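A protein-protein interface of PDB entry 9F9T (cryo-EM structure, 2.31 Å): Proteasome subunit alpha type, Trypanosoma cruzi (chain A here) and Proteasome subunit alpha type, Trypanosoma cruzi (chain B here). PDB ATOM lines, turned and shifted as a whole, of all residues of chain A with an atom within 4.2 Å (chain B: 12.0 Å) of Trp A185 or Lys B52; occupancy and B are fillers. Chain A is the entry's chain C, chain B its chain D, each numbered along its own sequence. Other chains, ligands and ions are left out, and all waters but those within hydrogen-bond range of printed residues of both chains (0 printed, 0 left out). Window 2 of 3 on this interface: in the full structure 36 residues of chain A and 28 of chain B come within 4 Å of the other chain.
NH1 of Arg A166 lies within hydrogen-bond range of O of Lys B52. The backbone NH (N) of Arg A166 is in hydrogen-bond range of the backbone carbonyl oxygen (O) of Leu B53.
O of Arg A166 lies within hydrogen-bond range of N of Leu A38 (2.8 Å). The backbone carbonyl oxygen (O) of Leu A38 lies within hydrogen-bond range of the indole nitrogen (NE1) of Trp A185 (3.0 Å). The indole nitrogen of Trp A185 sits at hydrogen-bond distance from the backbone carbonyl oxygen of Arg A166, 3.4 Å away.
Leu A38 touches Asp B55. Arg A166 touches Gln B54. Asp B55 touches Arg A166 (OD2 to CG, 3.5 Å). Arg A166 touches Ser B56 (NH2 to CB, 3.5 Å). Gln B51 touches Lys A182. Lys A182 touches Lys B52. Trp A185 touches Lys B52.
No residue of chain B comes within 4 Å of Ile A37. Arg A166 touches five residues of chain B. No residue of chain B comes within 4 Å of Leu A181. Trp A185 touches just one residue of chain B: Lys B52 (3.7 Å). No residue of chain B comes within 4 Å of Lys A186. No residue of chain B comes within 4 Å of Pro A187. No residue of chain B comes within 4 Å of Leu A189. Lys B48 touches none of the printed residues of chain A. Of chain A, only Arg A166 (2.6 Å), Lys A182 (3.0 Å) and Trp A185 (3.7 Å) come within 4 Å of Lys B52. Of the printed residues of chain A, Leu B53 touches Arg A166 (2.8 Å). Of the printed residues of chain A, Gln B54 touches Arg A166. Of the printed residues of chain A, Asp B55 touches Leu A38 (3.9 Å) and Arg A166 (3.5 Å). Printed residues of chain A within 4 Å of Ser B56: Arg A166 (3.5 Å). The nearest printed residue of chain A that does not touch Lys B52 is Arg A183 (4.5 Å).
Printed residues of chain B that touch a printed residue of chain A: Gln B51, Lys B52, Leu B53, Gln B54, Asp B55 and Ser B56. Along chain B the printed residues that touch a printed residue of chain A span positions 51 to 56. Of the 11 printed residues of chain A, 4 touch a printed residue of chain B. Printed residues of chain A that touch a printed residue of chain B: Leu A38, Arg A166, Lys A182 and Trp A185. Among the printed residues, no Asp or Glu carboxylate lies within 4 Å of a Lys or Arg side-chain nitrogen of the other chain.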
ATOM      1  N   ILE A  37      18.450  28.997   0.411  1.00  0.00           N
ATOM      2  CA  ILE A  37      18.046  29.451   1.733  1.00  0.00           C
ATOM      3  C   ILE A  37      16.996  28.563   2.409  1.00  0.00           C
ATOM      4  O   ILE A  37      15.908  28.371   1.883  1.00  0.00           O
ATOM      5  CB  ILE A  37      17.446  30.840   1.610  1.00  0.00           C
ATOM      6  CG1 ILE A  37      18.443  31.834   1.054  1.00  0.00           C
ATOM      7  CG2 ILE A  37      16.872  31.248   2.944  1.00  0.00           C
ATOM      8  CD1 ILE A  37      17.743  33.003   0.384  1.00  0.00           C
ATOM      9  N   LEU A  38      17.253  28.182   3.647  1.00  0.00           N
ATOM     10  CA  LEU A  38      16.307  27.454   4.472  1.00  0.00           C
ATOM     11  C   LEU A  38      15.355  28.415   5.194  1.00  0.00           C
ATOM     12  O   LEU A  38      15.786  29.323   5.894  1.00  0.00           O
ATOM     13  CB  LEU A  38      17.135  26.655   5.486  1.00  0.00           C
ATOM     14  CG  LEU A  38      16.369  25.608   6.289  1.00  0.00           C
ATOM     15  CD1 LEU A  38      15.832  24.551   5.349  1.00  0.00           C
ATOM     16  CD2 LEU A  38      17.245  24.950   7.350  1.00  0.00           C
ATOM     17  N   ARG A 166      21.991  26.484   6.341  1.00  0.00           N
ATOM     18  CA  ARG A 166      20.790  27.271   6.492  1.00  0.00           C
ATOM     19  C   ARG A 166      20.732  28.290   5.355  1.00  0.00           C
ATOM     20  O   ARG A 166      19.673  28.807   5.012  1.00  0.00           O
ATOM     21  CB  ARG A 166      20.897  28.004   7.831  1.00  0.00           C
ATOM     22  CG  ARG A 166      20.725  27.138   9.065  1.00  0.00           C
ATOM     23  CD  ARG A 166      21.372  27.836  10.248  1.00  0.00           C
ATOM     24  NE  ARG A 166      20.975  27.317  11.541  1.00  0.00           N
ATOM     25  CZ  ARG A 166      21.423  27.793  12.691  1.00  0.00           C
ATOM     26  NH1 ARG A 166      22.457  28.613  12.692  1.00  0.00           N
ATOM     27  NH2 ARG A 166      20.863  27.414  13.829  1.00  0.00           N
ATOM     28  N   LEU A 181      24.208  36.887   3.185  1.00  0.00           N
ATOM     29  CA  LEU A 181      23.242  35.978   3.781  1.00  0.00           C
ATOM     30  C   LEU A 181      23.490  35.926   5.282  1.00  0.00           C
ATOM     31  O   LEU A 181      22.547  35.944   6.065  1.00  0.00           O
ATOM     32  CB  LEU A 181      23.419  34.585   3.168  1.00  0.00           C
ATOM     33  CG  LEU A 181      23.014  34.438   1.708  1.00  0.00           C
ATOM     34  CD1 LEU A 181      23.603  33.158   1.139  1.00  0.00           C
ATOM     35  CD2 LEU A 181      21.499  34.466   1.556  1.00  0.00           C
ATOM     36  N   LYS A 182      24.783  35.827   5.629  1.00  0.00           N
ATOM     37  CA  LYS A 182      25.297  35.842   6.993  1.00  0.00           C
ATOM     38  C   LYS A 182      24.676  36.996   7.790  1.00  0.00           C
ATOM     39  O   LYS A 182      24.141  36.801   8.879  1.00  0.00           O
ATOM     40  CB  LYS A 182      26.822  35.934   6.886  1.00  0.00           C
ATOM     41  CG  LYS A 182      27.612  35.828   8.181  1.00  0.00           C
ATOM     42  CD  LYS A 182      29.066  35.458   7.940  1.00  0.00           C
ATOM     43  CE  LYS A 182      29.230  34.198   7.109  1.00  0.00           C
ATOM     44  NZ  LYS A 182      30.543  33.556   7.347  1.00  0.00           N
ATOM     45  N   ARG A 183      24.699  38.192   7.198  1.00  0.00           N
ATOM     46  CA  ARG A 183      24.108  39.364   7.809  1.00  0.00           C
ATOM     47  C   ARG A 183      22.590  39.190   7.958  1.00  0.00           C
ATOM     48  O   ARG A 183      22.070  39.337   9.063  1.00  0.00           O
ATOM     49  CB  ARG A 183      24.508  40.586   6.975  1.00  0.00           C
ATOM     50  CG  ARG A 183      24.189  41.928   7.614  1.00  0.00           C
ATOM     51  CD  ARG A 183      25.127  43.019   7.128  1.00  0.00           C
ATOM     52  NE  ARG A 183      25.167  43.177   5.679  1.00  0.00           N
ATOM     53  CZ  ARG A 183      24.160  43.618   4.928  1.00  0.00           C
ATOM     54  NH1 ARG A 183      22.968  43.830   5.458  1.00  0.00           N
ATOM     55  NH2 ARG A 183      24.346  43.839   3.637  1.00  0.00           N
ATOM     56  N   ASP A 184      21.880  38.831   6.875  1.00  0.00           N
ATOM     57  CA  ASP A 184      20.440  39.060   6.815  1.00  0.00           C
ATOM     58  C   ASP A 184      19.570  37.816   7.047  1.00  0.00           C
ATOM     59  O   ASP A 184      18.350  37.950   7.128  1.00  0.00           O
ATOM     60  CB  ASP A 184      20.068  39.766   5.508  1.00  0.00           C
ATOM     61  CG  ASP A 184      20.403  41.250   5.531  1.00  0.00           C
ATOM     62  OD1 ASP A 184      21.255  41.674   4.716  1.00  0.00           O
ATOM     63  OD2 ASP A 184      19.813  41.977   6.370  1.00  0.00           O
ATOM     64  N   TRP A 185      20.159  36.623   7.191  1.00  0.00           N
ATOM     65  CA  TRP A 185      19.384  35.422   7.471  1.00  0.00           C
ATOM     66  C   TRP A 185      18.964  35.458   8.935  1.00  0.00           C
ATOM     67  O   TRP A 185      19.657  36.034   9.766  1.00  0.00           O
ATOM     68  CB  TRP A 185      20.181  34.136   7.160  1.00  0.00           C
ATOM     69  CG  TRP A 185      19.405  32.850   7.336  1.00  0.00           C
ATOM     70  CD1 TRP A 185      18.630  32.242   6.389  1.00  0.00           C
ATOM     71  CD2 TRP A 185      19.277  32.033   8.530  1.00  0.00           C
ATOM     72  NE1 TRP A 185      18.046  31.108   6.893  1.00  0.00           N
ATOM     73  CE2 TRP A 185      18.418  30.951   8.203  1.00  0.00           C
ATOM     74  CE3 TRP A 185      19.792  32.097   9.832  1.00  0.00           C
ATOM     75  CZ2 TRP A 185      18.080  29.955   9.122  1.00  0.00           C
ATOM     76  CZ3 TRP A 185      19.454  31.112  10.744  1.00  0.00           C
ATOM     77  CH2 TRP A 185      18.603  30.063  10.396  1.00  0.00           C
ATOM     78  N   LYS A 186      17.842  34.806   9.239  1.00  0.00           N
ATOM     79  CA  LYS A 186      17.344  34.719  10.599  1.00  0.00           C
ATOM     80  C   LYS A 186      16.398  33.528  10.679  1.00  0.00           C
ATOM     81  O   LYS A 186      15.791  33.160   9.682  1.00  0.00           O
ATOM     82  CB  LYS A 186      16.670  36.041  10.979  1.00  0.00           C
ATOM     83  CG  LYS A 186      15.748  36.612   9.909  1.00  0.00           C
ATOM     84  CD  LYS A 186      15.972  38.093   9.638  1.00  0.00           C
ATOM     85  CE  LYS A 186      15.574  38.990  10.790  1.00  0.00           C
ATOM     86  NZ  LYS A 186      14.119  38.910  11.068  1.00  0.00           N
ATOM     87  N   PRO A 187      16.247  32.877  11.853  1.00  0.00           N
ATOM     88  CA  PRO A 187      15.530  31.605  11.932  1.00  0.00           C
ATOM     89  C   PRO A 187      14.001  31.667  11.943  1.00  0.00           C
ATOM     90  O   PRO A 187      13.351  30.710  12.374  1.00  0.00           O
ATOM     91  CB  PRO A 187      16.029  31.004  13.264  1.00  0.00           C
ATOM     92  CG  PRO A 187      17.133  31.935  13.758  1.00  0.00           C
ATOM     93  CD  PRO A 187      16.813  33.283  13.148  1.00  0.00           C
ATOM     94  N   LEU A 189      12.043  33.157   9.189  1.00  0.00           N
ATOM     95  CA  LEU A 189      11.657  33.635   7.867  1.00  0.00           C
ATOM     96  C   LEU A 189      10.395  32.918   7.383  1.00  0.00           C
ATOM     97  O   LEU A 189      10.265  31.705   7.534  1.00  0.00           O
ATOM     98  CB  LEU A 189      12.801  33.408   6.871  1.00  0.00           C
ATOM     99  CG  LEU A 189      13.977  34.382   6.884  1.00  0.00           C
ATOM    100  CD1 LEU A 189      15.101  33.877   5.975  1.00  0.00           C
ATOM    101  CD2 LEU A 189      13.554  35.780   6.456  1.00  0.00           C
ATOM    102  N   LYS B  47      35.620  20.226  15.022  1.00  0.00           N
ATOM    103  CA  LYS B  47      34.817  20.607  13.862  1.00  0.00           C
ATOM    104  C   LYS B  47      35.432  21.834  13.189  1.00  0.00           C
ATOM    105  O   LYS B  47      36.105  22.628  13.847  1.00  0.00           O
ATOM    106  CB  LYS B  47      33.378  20.937  14.264  1.00  0.00           C
ATOM    107  CG  LYS B  47      32.519  19.763  14.713  1.00  0.00           C
ATOM    108  CD  LYS B  47      31.674  20.075  15.950  1.00  0.00           C
ATOM    109  CE  LYS B  47      30.589  21.118  15.760  1.00  0.00           C
ATOM    110  NZ  LYS B  47      29.269  20.507  15.477  1.00  0.00           N
ATOM    111  N   LYS B  48      35.137  21.995  11.888  1.00  0.00           N
ATOM    112  CA  LYS B  48      35.778  22.980  11.024  1.00  0.00           C
ATOM    113  C   LYS B  48      35.895  24.332  11.724  1.00  0.00           C
ATOM    114  O   LYS B  48      37.000  24.782  12.020  1.00  0.00           O
ATOM    115  CB  LYS B  48      35.007  23.143   9.707  1.00  0.00           C
ATOM    116  CG  LYS B  48      35.192  22.023   8.688  1.00  0.00           C
ATOM    117  CD  LYS B  48      34.414  22.245   7.398  1.00  0.00           C
ATOM    118  CE  LYS B  48      35.091  23.182   6.417  1.00  0.00           C
ATOM    119  NZ  LYS B  48      36.190  22.507   5.686  1.00  0.00           N
ATOM    120  N   SER B  49      34.744  24.969  11.967  1.00  0.00           N
ATOM    121  CA  SER B  49      34.695  26.334  12.468  1.00  0.00           C
ATOM    122  C   SER B  49      33.233  26.751  12.620  1.00  0.00           C
ATOM    123  O   SER B  49      32.408  26.447  11.760  1.00  0.00           O
ATOM    124  CB  SER B  49      35.448  27.284  11.551  1.00  0.00           C
ATOM    125  OG  SER B  49      35.580  28.568  12.137  1.00  0.00           O
ATOM    126  N   VAL B  50      32.932  27.458  13.716  1.00  0.00           N
ATOM    127  CA  VAL B  50      31.572  27.881  14.027  1.00  0.00           C
ATOM    128  C   VAL B  50      31.115  28.899  12.984  1.00  0.00           C
ATOM    129  O   VAL B  50      31.808  29.882  12.726  1.00  0.00           O
ATOM    130  CB  VAL B  50      31.478  28.479  15.447  1.00  0.00           C
ATOM    131  CG1 VAL B  50      30.053  28.894  15.799  1.00  0.00           C
ATOM    132  CG2 VAL B  50      32.043  27.538  16.501  1.00  0.00           C
ATOM    133  N   GLN B  51      29.939  28.658  12.391  1.00  0.00           N
ATOM    134  CA  GLN B  51      29.331  29.612  11.480  1.00  0.00           C
ATOM    135  C   GLN B  51      27.875  29.818  11.877  1.00  0.00           C
ATOM    136  O   GLN B  51      27.269  28.972  12.535  1.00  0.00           O
ATOM    137  CB  GLN B  51      29.422  29.129  10.033  1.00  0.00           C
ATOM    138  CG  GLN B  51      30.838  28.776   9.608  1.00  0.00           C
ATOM    139  CD  GLN B  51      31.043  28.921   8.122  1.00  0.00           C
ATOM    140  OE1 GLN B  51      30.591  29.885   7.509  1.00  0.00           O
ATOM    141  NE2 GLN B  51      31.720  27.955   7.525  1.00  0.00           N
ATOM    142  N   LYS B  52      27.329  30.960  11.461  1.00  0.00           N
ATOM    143  CA  LYS B  52      25.927  31.269  11.677  1.00  0.00           C
ATOM    144  C   LYS B  52      25.091  30.361  10.774  1.00  0.00           C
ATOM    145  O   LYS B  52      23.977  29.977  11.119  1.00  0.00           O
ATOM    146  CB  LYS B  52      25.761  32.769  11.418  1.00  0.00           C
ATOM    147  CG  LYS B  52      24.386  33.371  11.666  1.00  0.00           C
ATOM    148  CD  LYS B  52      24.444  34.892  11.628  1.00  0.00           C
ATOM    149  CE  LYS B  52      23.114  35.563  11.361  1.00  0.00           C
ATOM    150  NZ  LYS B  52      22.156  35.356  12.471  1.00  0.00           N
ATOM    151  N   LEU B  53      25.681  29.979   9.634  1.00  0.00           N
ATOM    152  CA  LEU B  53      24.969  29.373   8.514  1.00  0.00           C
ATOM    153  C   LEU B  53      24.953  27.844   8.557  1.00  0.00           C
ATOM    154  O   LEU B  53      23.910  27.255   8.299  1.00  0.00           O
ATOM    155  CB  LEU B  53      25.659  29.842   7.236  1.00  0.00           C
ATOM    156  CG  LEU B  53      25.498  31.326   6.931  1.00  0.00           C
ATOM    157  CD1 LEU B  53      26.033  31.632   5.538  1.00  0.00           C
ATOM    158  CD2 LEU B  53      24.051  31.777   7.089  1.00  0.00           C
ATOM    159  N   GLN B  54      26.104  27.211   8.830  1.00  0.00           N
ATOM    160  CA  GLN B  54      26.178  25.800   9.204  1.00  0.00           C
ATOM    161  C   GLN B  54      24.933  25.403   9.973  1.00  0.00           C
ATOM    162  O   GLN B  54      24.369  26.225  10.665  1.00  0.00           O
ATOM    163  CB  GLN B  54      27.363  25.487  10.119  1.00  0.00           C
ATOM    164  CG  GLN B  54      27.935  24.098   9.881  1.00  0.00           C
ATOM    165  CD  GLN B  54      28.641  24.071   8.546  1.00  0.00           C
ATOM    166  OE1 GLN B  54      29.597  24.815   8.331  1.00  0.00           O
ATOM    167  NE2 GLN B  54      28.165  23.240   7.630  1.00  0.00           N
ATOM    168  N   ASP B  55      24.516  24.148   9.848  1.00  0.00           N
ATOM    169  CA  ASP B  55      23.249  23.731  10.424  1.00  0.00           C
ATOM    170  C   ASP B  55      23.504  23.284  11.864  1.00  0.00           C
ATOM    171  O   ASP B  55      24.384  22.463  12.109  1.00  0.00           O
ATOM    172  CB  ASP B  55      22.557  22.663   9.565  1.00  0.00           C
ATOM    173  CG  ASP B  55      21.039  22.677   9.699  1.00  0.00           C
ATOM    174  OD1 ASP B  55      20.470  21.694  10.221  1.00  0.00           O
ATOM    175  OD2 ASP B  55      20.434  23.677   9.288  1.00  0.00           O
ATOM    176  N   SER B  56      22.721  23.851  12.798  1.00  0.00           N
ATOM    177  CA  SER B  56      22.823  23.564  14.223  1.00  0.00           C
ATOM    178  C   SER B  56      22.889  22.054  14.477  1.00  0.00           C
ATOM    179  O   SER B  56      23.852  21.582  15.079  1.00  0.00           O
ATOM    180  CB  SER B  56      21.698  24.223  14.993  1.00  0.00           C
ATOM    181  OG  SER B  56      20.437  23.954  14.396  1.00  0.00           O
ATOM    182  N   ARG B  57      21.875  21.299  14.021  1.00  0.00           N
ATOM    183  CA  ARG B  57      22.015  19.856  13.879  1.00  0.00           C
ATOM    184  C   ARG B  57      23.087  19.605  12.825  1.00  0.00           C
ATOM    185  O   ARG B  57      22.780  19.426  11.649  1.00  0.00           O
ATOM    186  CB  ARG B  57      20.711  19.165  13.458  1.00  0.00           C
ATOM    187  CG  ARG B  57      20.851  17.659  13.262  1.00  0.00           C
ATOM    188  CD  ARG B  57      19.722  17.005  12.479  1.00  0.00           C
ATOM    189  NE  ARG B  57      19.743  17.211  11.028  1.00  0.00           N
ATOM    190  CZ  ARG B  57      20.571  16.614  10.170  1.00  0.00           C
ATOM    191  NH1 ARG B  57      20.384  16.749   8.868  1.00  0.00           N
ATOM    192  NH2 ARG B  57      21.560  15.853  10.610  1.00  0.00           N
ATOM    193  N   THR B  58      24.353  19.634  13.251  1.00  0.00           N
ATOM    194  CA  THR B  58      25.459  19.398  12.339  1.00  0.00           C
ATOM    195  C   THR B  58      25.488  17.917  11.963  1.00  0.00           C
ATOM    196  O   THR B  58      24.952  17.068  12.678  1.00  0.00           O
ATOM    197  CB  THR B  58      26.796  19.863  12.942  1.00  0.00           C
ATOM    198  OG1 THR B  58      26.899  19.285  14.244  1.00  0.00           O
ATOM    199  CG2 THR B  58      26.935  21.369  13.025  1.00  0.00           C
ATOM    200  N   SER B 201      34.080  26.346  22.013  1.00  0.00           N
ATOM    201  CA  SER B 201      32.660  26.652  22.092  1.00  0.00           C
ATOM    202  C   SER B 201      31.847  25.554  21.398  1.00  0.00           C
ATOM    203  O   SER B 201      31.304  24.675  22.071  1.00  0.00           O
ATOM    204  CB  SER B 201      32.383  28.035  21.537  1.00  0.00           C
ATOM    205  OG  SER B 201      31.019  28.390  21.703  1.00  0.00           O
ATOM    206  N   LYS B 202      31.786  25.601  20.057  1.00  0.00           N
ATOM    207  CA  LYS B 202      31.083  24.609  19.253  1.00  0.00           C
ATOM    208  C   LYS B 202      31.985  24.121  18.120  1.00  0.00           C
ATOM    209  O   LYS B 202      31.547  24.052  16.973  1.00  0.00           O
ATOM    210  CB  LYS B 202      29.817  25.184  18.600  1.00  0.00           C
ATOM    211  CG  LYS B 202      28.690  25.621  19.525  1.00  0.00           C
ATOM    212  CD  LYS B 202      27.537  26.233  18.757  1.00  0.00           C
ATOM    213  CE  LYS B 202      26.450  26.790  19.649  1.00  0.00           C
ATOM    214  NZ  LYS B 202      25.441  27.538  18.862  1.00  0.00           N
ATOM    215  N   ASN B 203      33.246  23.796  18.431  1.00  0.00           N
ATOM    216  CA  ASN B 203      34.107  23.153  17.449  1.00  0.00           C
ATOM    217  C   ASN B 203      34.657  21.850  18.041  1.00  0.00           C
ATOM    218  O   ASN B 203      35.801  21.466  17.782  1.00  0.00           O
ATOM    219  CB  ASN B 203      35.153  24.120  16.885  1.00  0.00           C
ATOM    220  CG  ASN B 203      35.952  24.846  17.943  1.00  0.00           C
ATOM    221  OD1 ASN B 203      35.725  24.662  19.136  1.00  0.00           O
ATOM    222  ND2 ASN B 203      36.883  25.682  17.508  1.00  0.00           N
